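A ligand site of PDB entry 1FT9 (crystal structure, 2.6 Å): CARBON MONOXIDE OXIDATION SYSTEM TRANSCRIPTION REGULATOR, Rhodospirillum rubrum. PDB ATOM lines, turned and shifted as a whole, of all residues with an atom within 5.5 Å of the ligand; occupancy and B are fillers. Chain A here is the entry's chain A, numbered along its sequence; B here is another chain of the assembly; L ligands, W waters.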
ATOM      1  N   PRO A   2     -22.061  20.412  16.061  1.00  0.00           N
ATOM      2  CA  PRO A   2     -20.653  20.153  16.406  1.00  0.00           C
ATOM      3  C   PRO A   2     -20.072  19.084  15.487  1.00  0.00           C
ATOM      4  O   PRO A   2     -20.801  18.243  14.973  1.00  0.00           O
ATOM      5  CB  PRO A   2     -20.715  19.656  17.847  1.00  0.00           C
ATOM      6  CG  PRO A   2     -22.043  20.150  18.349  1.00  0.00           C
ATOM      7  CD  PRO A   2     -22.938  19.981  17.165  1.00  0.00           C
ATOM      8  N   PRO A   3     -18.742  19.106  15.278  1.00  0.00           N
ATOM      9  CA  PRO A   3     -18.118  18.106  14.407  1.00  0.00           C
ATOM     10  C   PRO A   3     -18.105  16.802  15.179  1.00  0.00           C
ATOM     11  O   PRO A   3     -18.417  16.783  16.373  1.00  0.00           O
ATOM     12  CB  PRO A   3     -16.703  18.638  14.212  1.00  0.00           C
ATOM     13  CG  PRO A   3     -16.738  20.070  14.730  1.00  0.00           C
ATOM     14  CD  PRO A   3     -17.729  20.014  15.849  1.00  0.00           C
ATOM     15  N   ARG A   4     -17.782  15.691  14.509  1.00  0.00           N
ATOM     16  CA  ARG A   4     -17.702  14.443  15.256  1.00  0.00           C
ATOM     17  C   ARG A   4     -16.271  14.421  15.763  1.00  0.00           C
ATOM     18  O   ARG A   4     -15.397  15.113  15.231  1.00  0.00           O
ATOM     19  CB  ARG A   4     -18.027  13.230  14.380  1.00  0.00           C
ATOM     20  CG  ARG A   4     -19.542  13.086  14.177  1.00  0.00           C
ATOM     21  CD  ARG A   4     -19.928  11.734  13.608  1.00  0.00           C
ATOM     22  NE  ARG A   4     -20.994  11.855  12.613  1.00  0.00           N
ATOM     23  CZ  ARG A   4     -21.533  10.830  11.953  1.00  0.00           C
ATOM     24  NH1 ARG A   4     -21.123   9.589  12.191  1.00  0.00           N
ATOM     25  NH2 ARG A   4     -22.472  11.052  11.036  1.00  0.00           N
ATOM     26  N   TRP A 110     -13.237  18.444  22.764  1.00  0.00           N
ATOM     27  CA  TRP A 110     -14.091  18.175  21.626  1.00  0.00           C
ATOM     28  C   TRP A 110     -14.840  16.859  21.714  1.00  0.00           C
ATOM     29  O   TRP A 110     -15.874  16.673  21.070  1.00  0.00           O
ATOM     30  CB  TRP A 110     -13.284  18.284  20.341  1.00  0.00           C
ATOM     31  CG  TRP A 110     -12.943  19.704  20.082  1.00  0.00           C
ATOM     32  CD1 TRP A 110     -11.873  20.386  20.580  1.00  0.00           C
ATOM     33  CD2 TRP A 110     -13.746  20.652  19.379  1.00  0.00           C
ATOM     34  NE1 TRP A 110     -11.966  21.719  20.229  1.00  0.00           N
ATOM     35  CE2 TRP A 110     -13.100  21.898  19.487  1.00  0.00           C
ATOM     36  CE3 TRP A 110     -14.946  20.564  18.665  1.00  0.00           C
ATOM     37  CZ2 TRP A 110     -13.623  23.060  18.911  1.00  0.00           C
ATOM     38  CZ3 TRP A 110     -15.469  21.727  18.088  1.00  0.00           C
ATOM     39  CH2 TRP A 110     -14.806  22.952  18.223  1.00  0.00           C
ATOM     40  N   LEU A 120     -27.905  15.758  21.660  1.00  0.00           N
ATOM     41  CA  LEU A 120     -28.875  16.777  21.277  1.00  0.00           C
ATOM     42  C   LEU A 120     -29.692  16.387  20.040  1.00  0.00           C
ATOM     43  O   LEU A 120     -30.922  16.342  20.110  1.00  0.00           O
ATOM     44  CB  LEU A 120     -28.174  18.114  21.032  1.00  0.00           C
ATOM     45  CG  LEU A 120     -29.058  19.261  20.530  1.00  0.00           C
ATOM     46  CD1 LEU A 120     -30.137  19.561  21.560  1.00  0.00           C
ATOM     47  CD2 LEU A 120     -28.223  20.500  20.286  1.00  0.00           C
ATOM     48  N   THR A 121     -29.019  16.114  18.921  1.00  0.00           N
ATOM     49  CA  THR A 121     -29.731  15.754  17.693  1.00  0.00           C
ATOM     50  C   THR A 121     -30.599  14.520  17.909  1.00  0.00           C
ATOM     51  O   THR A 121     -31.703  14.433  17.383  1.00  0.00           O
ATOM     52  CB  THR A 121     -28.771  15.533  16.457  1.00  0.00           C
ATOM     53  OG1 THR A 121     -28.456  14.149  16.326  1.00  0.00           O
ATOM     54  CG2 THR A 121     -27.493  16.319  16.616  1.00  0.00           C
ATOM     55  N   MET A 124     -33.641  15.820  19.286  1.00  0.00           N
ATOM     56  CA  MET A 124     -34.402  16.590  18.314  1.00  0.00           C
ATOM     57  C   MET A 124     -35.153  15.606  17.437  1.00  0.00           C
ATOM     58  O   MET A 124     -36.318  15.822  17.096  1.00  0.00           O
ATOM     59  CB  MET A 124     -33.448  17.425  17.484  1.00  0.00           C
ATOM     60  CG  MET A 124     -32.634  18.337  18.327  1.00  0.00           C
ATOM     61  SD  MET A 124     -32.902  20.037  17.852  1.00  0.00           S
ATOM     62  CE  MET A 124     -31.377  20.370  16.948  1.00  0.00           C
ATOM     63  N   VAL B  44     -21.657  30.905  12.977  1.00  0.00           N
ATOM     64  CA  VAL B  44     -21.851  30.947  14.426  1.00  0.00           C
ATOM     65  C   VAL B  44     -21.993  32.386  14.890  1.00  0.00           C
ATOM     66  O   VAL B  44     -21.316  33.280  14.374  1.00  0.00           O
ATOM     67  CB  VAL B  44     -20.653  30.316  15.144  1.00  0.00           C
ATOM     68  CG1 VAL B  44     -20.800  30.481  16.638  1.00  0.00           C
ATOM     69  CG2 VAL B  44     -20.546  28.859  14.801  1.00  0.00           C
ATOM     70  N   MET B  73     -23.766  31.845  22.697  1.00  0.00           N
ATOM     71  CA  MET B  73     -23.288  31.557  21.353  1.00  0.00           C
ATOM     72  C   MET B  73     -24.219  30.518  20.770  1.00  0.00           C
ATOM     73  O   MET B  73     -24.835  29.735  21.511  1.00  0.00           O
ATOM     74  CB  MET B  73     -21.856  31.006  21.374  1.00  0.00           C
ATOM     75  CG  MET B  73     -20.865  31.986  21.986  1.00  0.00           C
ATOM     76  SD  MET B  73     -19.179  31.357  22.198  1.00  0.00           S
ATOM     77  CE  MET B  73     -19.493  29.824  23.065  1.00  0.00           C
ATOM     78  N   PHE B  74     -24.378  30.539  19.457  1.00  0.00           N
ATOM     79  CA  PHE B  74     -25.235  29.566  18.789  1.00  0.00           C
ATOM     80  C   PHE B  74     -24.849  29.510  17.329  1.00  0.00           C
ATOM     81  O   PHE B  74     -24.064  30.358  16.852  1.00  0.00           O
ATOM     82  CB  PHE B  74     -26.711  29.954  18.919  1.00  0.00           C
ATOM     83  CG  PHE B  74     -27.648  28.802  18.797  1.00  0.00           C
ATOM     84  CD1 PHE B  74     -27.599  27.762  19.714  1.00  0.00           C
ATOM     85  CD2 PHE B  74     -28.614  28.766  17.785  1.00  0.00           C
ATOM     86  CE1 PHE B  74     -28.497  26.690  19.631  1.00  0.00           C
ATOM     87  CE2 PHE B  74     -29.515  27.706  17.683  1.00  0.00           C
ATOM     88  CZ  PHE B  74     -29.466  26.664  18.611  1.00  0.00           C
ATOM     89  N   CYS B  75     -25.402  28.530  16.626  1.00  0.00           N
ATOM     90  CA  CYS B  75     -25.073  28.353  15.223  1.00  0.00           C
ATOM     91  C   CYS B  75     -26.258  28.558  14.275  1.00  0.00           C
ATOM     92  O   CYS B  75     -27.386  28.805  14.714  1.00  0.00           O
ATOM     93  CB  CYS B  75     -24.531  26.945  15.008  1.00  0.00           C
ATOM     94  SG  CYS B  75     -25.855  25.730  15.086  1.00  0.00           S
ATOM     95  N   HIS B  77     -27.080  26.135  12.005  1.00  0.00           N
ATOM     96  CA  HIS B  77     -27.407  24.831  11.450  1.00  0.00           C
ATOM     97  C   HIS B  77     -28.025  23.851  12.447  1.00  0.00           C
ATOM     98  O   HIS B  77     -27.991  22.635  12.251  1.00  0.00           O
ATOM     99  CB  HIS B  77     -26.151  24.194  10.841  1.00  0.00           C
ATOM    100  CG  HIS B  77     -25.037  23.984  11.823  1.00  0.00           C
ATOM    101  ND1 HIS B  77     -24.016  24.890  11.999  1.00  0.00           N
ATOM    102  CD2 HIS B  77     -24.797  22.968  12.684  1.00  0.00           C
ATOM    103  CE1 HIS B  77     -23.183  24.435  12.920  1.00  0.00           C
ATOM    104  NE2 HIS B  77     -23.633  23.274  13.349  1.00  0.00           N
ATOM    105  N   SER B  78     -28.583  24.365  13.532  1.00  0.00           N
ATOM    106  CA  SER B  78     -29.184  23.505  14.534  1.00  0.00           C
ATOM    107  C   SER B  78     -30.390  22.784  13.947  1.00  0.00           C
ATOM    108  O   SER B  78     -30.703  21.653  14.313  1.00  0.00           O
ATOM    109  CB  SER B  78     -29.596  24.328  15.755  1.00  0.00           C
ATOM    110  OG  SER B  78     -30.532  25.342  15.400  1.00  0.00           O
ATOM    111  N   GLY B  79     -31.059  23.459  13.018  1.00  0.00           N
ATOM    112  CA  GLY B  79     -32.261  22.900  12.412  1.00  0.00           C
ATOM    113  C   GLY B  79     -33.448  23.583  13.064  1.00  0.00           C
ATOM    114  O   GLY B  79     -34.554  23.602  12.531  1.00  0.00           O
ATOM    115  N   ILE B  95     -18.223  29.227  10.400  1.00  0.00           N
ATOM    116  CA  ILE B  95     -17.697  28.127  11.197  1.00  0.00           C
ATOM    117  C   ILE B  95     -16.172  28.061  11.199  1.00  0.00           C
ATOM    118  O   ILE B  95     -15.555  27.870  12.246  1.00  0.00           O
ATOM    119  CB  ILE B  95     -18.202  26.787  10.665  1.00  0.00           C
ATOM    120  CG1 ILE B  95     -19.716  26.716  10.826  1.00  0.00           C
ATOM    121  CG2 ILE B  95     -17.512  25.663  11.391  1.00  0.00           C
ATOM    122  CD1 ILE B  95     -20.192  26.897  12.257  1.00  0.00           C
ATOM    123  N   PHE B  98     -14.707  30.672  13.515  1.00  0.00           N
ATOM    124  CA  PHE B  98     -15.011  30.352  14.900  1.00  0.00           C
ATOM    125  C   PHE B  98     -14.093  29.233  15.424  1.00  0.00           C
ATOM    126  O   PHE B  98     -13.475  29.347  16.482  1.00  0.00           O
ATOM    127  CB  PHE B  98     -16.483  29.939  15.033  1.00  0.00           C
ATOM    128  CG  PHE B  98     -16.945  29.725  16.450  1.00  0.00           C
ATOM    129  CD1 PHE B  98     -16.690  30.691  17.427  1.00  0.00           C
ATOM    130  CD2 PHE B  98     -17.626  28.568  16.809  1.00  0.00           C
ATOM    131  CE1 PHE B  98     -17.104  30.494  18.753  1.00  0.00           C
ATOM    132  CE2 PHE B  98     -18.038  28.363  18.124  1.00  0.00           C
ATOM    133  CZ  PHE B  98     -17.783  29.329  19.101  1.00  0.00           C
ATOM    134  N   GLU B  99     -13.989  28.156  14.647  1.00  0.00           N
ATOM    135  CA  GLU B  99     -13.152  27.022  15.031  1.00  0.00           C
ATOM    136  C   GLU B  99     -11.700  27.441  15.173  1.00  0.00           C
ATOM    137  O   GLU B  99     -11.002  26.979  16.078  1.00  0.00           O
ATOM    138  CB  GLU B  99     -13.277  25.902  14.007  1.00  0.00           C
ATOM    139  CG  GLU B  99     -12.338  24.742  14.281  1.00  0.00           C
ATOM    140  CD  GLU B  99     -12.701  23.517  13.476  1.00  0.00           C
ATOM    141  OE1 GLU B  99     -13.006  23.677  12.279  1.00  0.00           O
ATOM    142  OE2 GLU B  99     -12.665  22.408  14.051  1.00  0.00           O
ATOM    143  N   LEU B 102     -11.402  29.230  18.431  1.00  0.00           N
ATOM    144  CA  LEU B 102     -11.496  28.248  19.515  1.00  0.00           C
ATOM    145  C   LEU B 102     -10.189  27.492  19.666  1.00  0.00           C
ATOM    146  O   LEU B 102      -9.818  27.080  20.775  1.00  0.00           O
ATOM    147  CB  LEU B 102     -12.629  27.258  19.251  1.00  0.00           C
ATOM    148  CG  LEU B 102     -14.042  27.788  19.479  1.00  0.00           C
ATOM    149  CD1 LEU B 102     -15.049  26.760  19.022  1.00  0.00           C
ATOM    150  CD2 LEU B 102     -14.241  28.120  20.957  1.00  0.00           C
ATOM    151  N   LEU B 112     -19.407  26.944  24.217  1.00  0.00           N
ATOM    152  CA  LEU B 112     -20.084  26.094  23.235  1.00  0.00           C
ATOM    153  C   LEU B 112     -20.650  24.873  23.974  1.00  0.00           C
ATOM    154  O   LEU B 112     -21.789  24.457  23.738  1.00  0.00           O
ATOM    155  CB  LEU B 112     -19.106  25.645  22.149  1.00  0.00           C
ATOM    156  CG  LEU B 112     -19.570  24.577  21.147  1.00  0.00           C
ATOM    157  CD1 LEU B 112     -20.699  25.113  20.281  1.00  0.00           C
ATOM    158  CD2 LEU B 112     -18.377  24.179  20.291  1.00  0.00           C
ATOM    159  N   ILE B 115     -23.877  25.928  25.912  1.00  0.00           N
ATOM    160  CA  ILE B 115     -25.089  26.088  25.140  1.00  0.00           C
ATOM    161  C   ILE B 115     -25.621  24.736  24.699  1.00  0.00           C
ATOM    162  O   ILE B 115     -26.830  24.518  24.695  1.00  0.00           O
ATOM    163  CB  ILE B 115     -24.908  27.020  23.925  1.00  0.00           C
ATOM    164  CG1 ILE B 115     -26.279  27.537  23.482  1.00  0.00           C
ATOM    165  CG2 ILE B 115     -24.251  26.284  22.765  1.00  0.00           C
ATOM    166  CD1 ILE B 115     -26.964  28.397  24.529  1.00  0.00           C
ATOM    167  N   LEU B 116     -24.732  23.800  24.360  1.00  0.00           N
ATOM    168  CA  LEU B 116     -25.180  22.480  23.950  1.00  0.00           C
ATOM    169  C   LEU B 116     -25.878  21.770  25.098  1.00  0.00           C
ATOM    170  O   LEU B 116     -26.874  21.088  24.890  1.00  0.00           O
ATOM    171  CB  LEU B 116     -24.002  21.623  23.456  1.00  0.00           C
ATOM    172  CG  LEU B 116     -23.386  21.980  22.102  1.00  0.00           C
ATOM    173  CD1 LEU B 116     -21.973  21.386  21.947  1.00  0.00           C
ATOM    174  CD2 LEU B 116     -24.329  21.489  20.999  1.00  0.00           C
HETATM  175  C1  LIG L   1     -24.256  19.233  13.205  1.00  0.00           C
HETATM  176  C2  LIG L   1     -25.804  22.250  16.654  1.00  0.00           C
HETATM  177  C3  LIG L   1     -21.551  24.523  16.564  1.00  0.00           C
HETATM  178  C4  LIG L   1     -20.090  21.583  12.988  1.00  0.00           C
HETATM  179  C5  LIG L   1     -24.978  19.800  14.234  1.00  0.00           C
HETATM  180  C6  LIG L   1     -26.308  19.405  14.605  1.00  0.00           C
HETATM  181  C7  LIG L   1     -26.771  20.288  15.534  1.00  0.00           C
HETATM  182  C8  LIG L   1     -25.732  21.242  15.706  1.00  0.00           C
HETATM  183  C9  LIG L   1     -28.109  20.302  16.254  1.00  0.00           C
HETATM  184  C10 LIG L   1     -27.148  18.305  13.980  1.00  0.00           C
HETATM  185  C11 LIG L   1     -27.703  18.699  12.614  1.00  0.00           C
HETATM  186  C12 LIG L   1     -29.036  18.025  12.301  1.00  0.00           C
HETATM  187  O1  LIG L   1     -30.040  18.313  13.003  1.00  0.00           O
HETATM  188  O2  LIG L   1     -29.064  17.208  11.354  1.00  0.00           O
HETATM  189  C13 LIG L   1     -24.774  23.098  16.953  1.00  0.00           C
HETATM  190  C14 LIG L   1     -24.858  24.113  17.973  1.00  0.00           C
HETATM  191  C15 LIG L   1     -23.749  24.862  17.893  1.00  0.00           C
HETATM  192  C16 LIG L   1     -22.886  24.208  16.886  1.00  0.00           C
HETATM  193  C17 LIG L   1     -25.915  24.169  19.060  1.00  0.00           C
HETATM  194  C18 LIG L   1     -23.536  25.965  18.719  1.00  0.00           C
HETATM  195  C19 LIG L   1     -22.556  27.035  18.485  1.00  0.00           C
HETATM  196  C20 LIG L   1     -20.773  23.871  15.581  1.00  0.00           C
HETATM  197  C21 LIG L   1     -19.337  24.131  15.338  1.00  0.00           C
HETATM  198  C22 LIG L   1     -18.942  23.293  14.328  1.00  0.00           C
HETATM  199  C23 LIG L   1     -20.126  22.543  13.978  1.00  0.00           C
HETATM  200  C24 LIG L   1     -18.422  25.085  16.112  1.00  0.00           C
HETATM  201  C25 LIG L   1     -17.676  23.073  13.776  1.00  0.00           C
HETATM  202  C26 LIG L   1     -16.350  23.365  14.370  1.00  0.00           C
HETATM  203  C27 LIG L   1     -21.126  20.756  12.681  1.00  0.00           C
HETATM  204  C28 LIG L   1     -20.996  19.693  11.723  1.00  0.00           C
HETATM  205  C29 LIG L   1     -22.212  19.051  11.713  1.00  0.00           C
HETATM  206  C30 LIG L   1     -23.026  19.684  12.755  1.00  0.00           C
HETATM  207  C31 LIG L   1     -19.680  19.306  11.045  1.00  0.00           C
HETATM  208  C32 LIG L   1     -22.617  17.927  10.781  1.00  0.00           C
HETATM  209  C33 LIG L   1     -21.765  16.670  10.824  1.00  0.00           C
HETATM  210  C34 LIG L   1     -21.930  15.859  12.106  1.00  0.00           C
HETATM  211  O3  LIG L   1     -21.518  16.340  13.183  1.00  0.00           O
HETATM  212  O4  LIG L   1     -22.490  14.740  12.031  1.00  0.00           O
HETATM  213  N1  LIG L   1     -24.612  20.948  14.928  1.00  0.00           N
HETATM  214  N2  LIG L   1     -23.561  23.119  16.305  1.00  0.00           N
HETATM  215  N3  LIG L   1     -21.217  22.845  14.766  1.00  0.00           N
HETATM  216  N4  LIG L   1     -22.339  20.733  13.340  1.00  0.00           N
HETATM  217 FE1  LIG L   1     -22.924  21.927  14.831  1.00  0.00          FE
HETATM  218  O   HOH W   1     -23.021  17.133  15.642  1.00  0.00           O
HETATM  219  O   HOH W   2     -23.054  17.805   8.027  1.00  0.00           O
HETATM  220  O   HOH W   3     -18.581  15.960  10.946  1.00  0.00           O
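Water W1 bridges the backbone carbonyl oxygen (O) of Pro 2 (2.6 Å) and an oxygen (O3) of the ligand (3.0 Å).
A ring nitrogen (NE2) of His 77 of chain B is bound to an iron atom (FE1) of the ligand (2.1 Å). N of Pro 2 is bound to FE1 of the ligand. O of Pro 2 sits close to O3 of the ligand (2.7 Å). The guanidinium group (NE) of Arg 4 lies within salt-bridge range of an oxygen (O4) of the ligand (3.3 Å).
SG of Cys 75 of chain B sits close to N2 of the ligand, 3.7 Å away. CG of Pro 3 touches C25 of the ligand, at 3.3 Å. Thr 121 touches the ligand. Met 124 touches the ligand. Phe 74 of chain B touches the ligand (C to C19, 3.6 Å). O of Ser 78 of chain B touches C9 of the ligand (3.5 Å). Ile 95 of chain B touches the ligand. Phe 98 of chain B touches the ligand (CD2 to C24, 3.6 Å). Glu 99 of chain B touches the ligand. CD1 of Leu 112 of chain B touches C19 of the ligand, 3.2 Å away. Leu 116 of chain B touches the ligand. Within 4 Å of the ligand: Pro 2, Pro 3, Arg 4, Thr 121, Met 124, Phe 74 of chain B, Cys 75 of chain B, His 77 of chain B, Ser 78 of chain B, Ile 95 of chain B, Phe 98 of chain B, Glu 99 of chain B, Leu 112 of chain B and Leu 116 of chain B. The nearest printed residue that does not touch the ligand is Leu 120 (4.04 Å).
N of His 77 of chain B is in hydrogen-bond range of SG of Cys 75 of chain B. N of Ser 78 of chain B sits at hydrogen-bond distance from SG of Cys 75 of chain B.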
